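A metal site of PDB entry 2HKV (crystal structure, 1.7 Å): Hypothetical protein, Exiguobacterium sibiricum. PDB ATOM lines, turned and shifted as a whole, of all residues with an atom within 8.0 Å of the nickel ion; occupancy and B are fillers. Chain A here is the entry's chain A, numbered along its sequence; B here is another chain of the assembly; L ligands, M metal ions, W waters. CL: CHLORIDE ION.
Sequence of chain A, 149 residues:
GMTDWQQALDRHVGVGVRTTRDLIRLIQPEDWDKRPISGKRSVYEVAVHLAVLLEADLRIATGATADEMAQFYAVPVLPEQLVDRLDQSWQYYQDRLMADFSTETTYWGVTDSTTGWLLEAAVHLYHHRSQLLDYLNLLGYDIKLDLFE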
ATOM      1  N   ARG A  41      -4.953 -14.562 -24.415  1.00  0.00           N
ATOM      2  CA  ARG A  41      -5.904 -13.621 -23.815  1.00  0.00           C
ATOM      3  C   ARG A  41      -7.353 -14.092 -24.063  1.00  0.00           C
ATOM      4  O   ARG A  41      -7.666 -14.703 -25.083  1.00  0.00           O
ATOM      5  CB  ARG A  41      -5.717 -12.247 -24.417  1.00  0.00           C
ATOM      6  CG  ARG A  41      -4.691 -11.311 -23.769  1.00  0.00           C
ATOM      7  CD  ARG A  41      -4.407 -10.185 -24.673  1.00  0.00           C
ATOM      8  NE  ARG A  41      -3.765  -9.067 -23.998  1.00  0.00           N
ATOM      9  CZ  ARG A  41      -2.487  -8.750 -24.167  1.00  0.00           C
ATOM     10  NH1 ARG A  41      -1.742  -9.427 -25.038  1.00  0.00           N
ATOM     11  NH2 ARG A  41      -1.941  -7.738 -23.495  1.00  0.00           N
ATOM     12  N   VAL A  46      -8.471  -9.254 -24.897  1.00  0.00           N
ATOM     13  CA  VAL A  46      -8.135  -8.715 -26.217  1.00  0.00           C
ATOM     14  C   VAL A  46      -8.806  -7.375 -26.442  1.00  0.00           C
ATOM     15  O   VAL A  46      -8.174  -6.421 -26.889  1.00  0.00           O
ATOM     16  CB  VAL A  46      -8.506  -9.659 -27.341  1.00  0.00           C
ATOM     17  CG1 VAL A  46      -7.995  -9.109 -28.716  1.00  0.00           C
ATOM     18  CG2 VAL A  46      -7.800 -10.976 -27.151  1.00  0.00           C
ATOM     19  N   HIS A  49      -7.238  -4.453 -24.444  1.00  0.00           N
ATOM     20  CA  HIS A  49      -5.905  -4.101 -25.006  1.00  0.00           C
ATOM     21  C   HIS A  49      -6.149  -3.259 -26.260  1.00  0.00           C
ATOM     22  O   HIS A  49      -5.543  -2.193 -26.432  1.00  0.00           O
ATOM     23  CB  HIS A  49      -5.104  -5.384 -25.272  1.00  0.00           C
ATOM     24  CG  HIS A  49      -3.725  -5.200 -25.879  1.00  0.00           C
ATOM     25  ND1 HIS A  49      -2.753  -4.408 -25.319  1.00  0.00           N
ATOM     26  CD2 HIS A  49      -3.123  -5.821 -26.940  1.00  0.00           C
ATOM     27  CE1 HIS A  49      -1.631  -4.516 -26.012  1.00  0.00           C
ATOM     28  NE2 HIS A  49      -1.839  -5.323 -27.041  1.00  0.00           N
ATOM     29  N   LEU A  50      -7.065  -3.700 -27.122  1.00  0.00           N
ATOM     30  CA  LEU A  50      -7.455  -2.909 -28.317  1.00  0.00           C
ATOM     31  C   LEU A  50      -7.992  -1.492 -27.969  1.00  0.00           C
ATOM     32  O   LEU A  50      -7.637  -0.481 -28.617  1.00  0.00           O
ATOM     33  CB  LEU A  50      -8.515  -3.670 -29.096  1.00  0.00           C
ATOM     34  CG  LEU A  50      -8.099  -4.660 -30.168  1.00  0.00           C
ATOM     35  CD1 LEU A  50      -9.299  -5.635 -30.467  1.00  0.00           C
ATOM     36  CD2 LEU A  50      -7.615  -3.899 -31.442  1.00  0.00           C
ATOM     37  N   LEU A  53      -4.754   0.593 -26.678  1.00  0.00           N
ATOM     38  CA  LEU A  53      -3.396   0.560 -27.172  1.00  0.00           C
ATOM     39  C   LEU A  53      -2.961   1.815 -27.964  1.00  0.00           C
ATOM     40  O   LEU A  53      -1.759   2.108 -28.046  1.00  0.00           O
ATOM     41  CB  LEU A  53      -3.090  -0.722 -27.942  1.00  0.00           C
ATOM     42  CG  LEU A  53      -3.723  -1.020 -29.302  1.00  0.00           C
ATOM     43  CD1 LEU A  53      -3.125  -0.199 -30.544  1.00  0.00           C
ATOM     44  CD2 LEU A  53      -3.567  -2.544 -29.540  1.00  0.00           C
ATOM     45  N   ASP A  57       0.541   3.037 -26.574  1.00  0.00           N
ATOM     46  CA  ASP A  57       1.762   3.032 -27.348  1.00  0.00           C
ATOM     47  C   ASP A  57       2.361   4.407 -27.458  1.00  0.00           C
ATOM     48  O   ASP A  57       3.580   4.543 -27.483  1.00  0.00           O
ATOM     49  CB  ASP A  57       1.540   2.446 -28.757  1.00  0.00           C
ATOM     50  CG  ASP A  57       1.293   0.921 -28.759  1.00  0.00           C
ATOM     51  OD1 ASP A  57       1.058   0.276 -27.682  1.00  0.00           O
ATOM     52  OD2 ASP A  57       1.303   0.326 -29.873  1.00  0.00           O
ATOM     53  N   TYR A  73      -2.245   0.563 -17.218  1.00  0.00           N
ATOM     54  CA  TYR A  73      -2.865  -0.697 -17.523  1.00  0.00           C
ATOM     55  C   TYR A  73      -3.762  -1.176 -16.431  1.00  0.00           C
ATOM     56  O   TYR A  73      -4.690  -1.915 -16.707  1.00  0.00           O
ATOM     57  CB  TYR A  73      -1.810  -1.762 -17.832  1.00  0.00           C
ATOM     58  CG  TYR A  73      -1.031  -1.529 -19.088  1.00  0.00           C
ATOM     59  CD1 TYR A  73      -1.680  -1.259 -20.289  1.00  0.00           C
ATOM     60  CD2 TYR A  73       0.352  -1.582 -19.095  1.00  0.00           C
ATOM     61  CE1 TYR A  73      -0.976  -1.073 -21.462  1.00  0.00           C
ATOM     62  CE2 TYR A  73       1.067  -1.377 -20.275  1.00  0.00           C
ATOM     63  CZ  TYR A  73       0.398  -1.119 -21.448  1.00  0.00           C
ATOM     64  OH  TYR A  73       1.066  -0.935 -22.622  1.00  0.00           O
ATOM     65  N   GLU A 120       3.630   2.365 -35.818  1.00  0.00           N
ATOM     66  CA  GLU A 120       3.663   1.192 -34.970  1.00  0.00           C
ATOM     67  C   GLU A 120       2.319   0.976 -34.301  1.00  0.00           C
ATOM     68  O   GLU A 120       1.855  -0.143 -34.214  1.00  0.00           O
ATOM     69  CB  GLU A 120       4.766   1.313 -33.914  1.00  0.00           C
ATOM     70  CG  GLU A 120       5.035   0.078 -33.034  1.00  0.00           C
ATOM     71  CD  GLU A 120       3.938  -0.166 -31.973  1.00  0.00           C
ATOM     72  OE1 GLU A 120       3.336   0.818 -31.512  1.00  0.00           O
ATOM     73  OE2 GLU A 120       3.691  -1.326 -31.558  1.00  0.00           O
ATOM     74  N   HIS A 124      -0.075  -2.285 -34.836  1.00  0.00           N
ATOM     75  CA  HIS A 124      -0.472  -2.973 -33.602  1.00  0.00           C
ATOM     76  C   HIS A 124      -2.002  -3.102 -33.450  1.00  0.00           C
ATOM     77  O   HIS A 124      -2.549  -4.178 -33.152  1.00  0.00           O
ATOM     78  CB  HIS A 124       0.192  -2.234 -32.424  1.00  0.00           C
ATOM     79  CG  HIS A 124       0.097  -2.935 -31.133  1.00  0.00           C
ATOM     80  ND1 HIS A 124       0.332  -2.294 -29.942  1.00  0.00           N
ATOM     81  CD2 HIS A 124      -0.234  -4.213 -30.838  1.00  0.00           C
ATOM     82  CE1 HIS A 124       0.158  -3.161 -28.962  1.00  0.00           C
ATOM     83  NE2 HIS A 124      -0.168  -4.313 -29.493  1.00  0.00           N
ATOM     84  N   LEU A 125      -2.713  -2.062 -33.833  1.00  0.00           N
ATOM     85  CA  LEU A 125      -4.165  -2.087 -33.874  1.00  0.00           C
ATOM     86  C   LEU A 125      -4.735  -3.151 -34.845  1.00  0.00           C
ATOM     87  O   LEU A 125      -5.608  -3.973 -34.447  1.00  0.00           O
ATOM     88  CB  LEU A 125      -4.743  -0.689 -34.211  1.00  0.00           C
ATOM     89  CG  LEU A 125      -6.275  -0.590 -34.147  1.00  0.00           C
ATOM     90  CD1 LEU A 125      -6.764  -0.514 -32.701  1.00  0.00           C
ATOM     91  CD2 LEU A 125      -6.749   0.648 -34.988  1.00  0.00           C
ATOM     92  N   HIS A 127      -3.097  -5.759 -35.969  1.00  0.00           N
ATOM     93  CA  HIS A 127      -2.720  -7.074 -35.392  1.00  0.00           C
ATOM     94  C   HIS A 127      -3.824  -7.603 -34.449  1.00  0.00           C
ATOM     95  O   HIS A 127      -4.277  -8.740 -34.551  1.00  0.00           O
ATOM     96  CB  HIS A 127      -1.373  -6.951 -34.672  1.00  0.00           C
ATOM     97  CG  HIS A 127      -0.954  -8.158 -33.878  1.00  0.00           C
ATOM     98  ND1 HIS A 127      -0.373  -9.266 -34.473  1.00  0.00           N
ATOM     99  CD2 HIS A 127      -1.050  -8.451 -32.563  1.00  0.00           C
ATOM    100  CE1 HIS A 127      -0.112 -10.182 -33.545  1.00  0.00           C
ATOM    101  NE2 HIS A 127      -0.524  -9.713 -32.374  1.00  0.00           N
ATOM    102  N   HIS A 128      -4.237  -6.791 -33.482  1.00  0.00           N
ATOM    103  CA  HIS A 128      -5.195  -7.251 -32.538  1.00  0.00           C
ATOM    104  C   HIS A 128      -6.629  -7.222 -33.032  1.00  0.00           C
ATOM    105  O   HIS A 128      -7.429  -8.034 -32.537  1.00  0.00           O
ATOM    106  CB  HIS A 128      -5.088  -6.554 -31.192  1.00  0.00           C
ATOM    107  CG  HIS A 128      -3.817  -6.856 -30.463  1.00  0.00           C
ATOM    108  ND1 HIS A 128      -3.532  -8.109 -29.975  1.00  0.00           N
ATOM    109  CD2 HIS A 128      -2.814  -6.056 -30.093  1.00  0.00           C
ATOM    110  CE1 HIS A 128      -2.371  -8.038 -29.323  1.00  0.00           C
ATOM    111  NE2 HIS A 128      -1.878  -6.814 -29.443  1.00  0.00           N
ATOM    112  N   GLN A 131      -6.907 -10.577 -34.410  1.00  0.00           N
ATOM    113  CA  GLN A 131      -7.049 -11.562 -33.334  1.00  0.00           C
ATOM    114  C   GLN A 131      -8.510 -11.642 -32.871  1.00  0.00           C
ATOM    115  O   GLN A 131      -9.074 -12.767 -32.727  1.00  0.00           O
ATOM    116  CB  GLN A 131      -6.197 -11.157 -32.161  1.00  0.00           C
ATOM    117  CG  GLN A 131      -6.088 -12.171 -31.085  1.00  0.00           C
ATOM    118  CD  GLN A 131      -5.042 -11.798 -30.057  1.00  0.00           C
ATOM    119  OE1 GLN A 131      -4.414 -10.745 -30.136  1.00  0.00           O
ATOM    120  NE2 GLN A 131      -4.829 -12.694 -29.058  1.00  0.00           N
ATOM    121  N   PHE B 148       6.991  -7.577 -32.355  1.00  0.00           N
ATOM    122  CA  PHE B 148       7.249  -6.145 -32.385  1.00  0.00           C
ATOM    123  C   PHE B 148       8.590  -5.917 -31.690  1.00  0.00           C
ATOM    124  O   PHE B 148       9.152  -4.809 -31.713  1.00  0.00           O
ATOM    125  CB  PHE B 148       6.119  -5.375 -31.666  1.00  0.00           C
ATOM    126  CG  PHE B 148       4.768  -5.427 -32.372  1.00  0.00           C
ATOM    127  CD1 PHE B 148       4.430  -4.471 -33.355  1.00  0.00           C
ATOM    128  CD2 PHE B 148       3.833  -6.422 -32.041  1.00  0.00           C
ATOM    129  CE1 PHE B 148       3.189  -4.524 -33.982  1.00  0.00           C
ATOM    130  CE2 PHE B 148       2.590  -6.477 -32.677  1.00  0.00           C
ATOM    131  CZ  PHE B 148       2.274  -5.530 -33.653  1.00  0.00           C
HETATM  132 CL    CL L   1       1.005  -6.868 -29.213  1.00  0.00          CL
HETATM  133 NI    NI M   1      -0.401  -6.030 -28.243  1.00  0.00          NI
HETATM  134  O   HOH W   1      -0.295  -7.926 -27.030  1.00  0.00           O
HETATM  135  O   HOH W   2       1.169  -5.424 -27.020  1.00  0.00           O
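A ring nitrogen (ND1) of His 124 is in hydrogen-bond range of the side-chain carboxylate of Asp 57 (2.8 Å).
The side-chain amide oxygen (OE1) of Gln 131 is in hydrogen-bond range of a ring nitrogen (ND1) of His 128, 2.8 Å away.
Along chain A the residues within 4 Å of the nickel ion span positions 49 to 128.
The nearest printed residue that does not touch the nickel ion is Arg 41 (4.9 Å).
The nickel ion is bound by CL of the ligand (1.9 Å).
NE2 of His 49 is bound to the nickel ion, 2.0 Å away.
The nickel ion is bound by NE2 of His 128 (2.1 Å).
The nickel ion is bound by water W2 (2.1 Å).
NE2 of His 124 binds the nickel ion.
Water W1 binds the nickel ion, at 2.3 Å.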
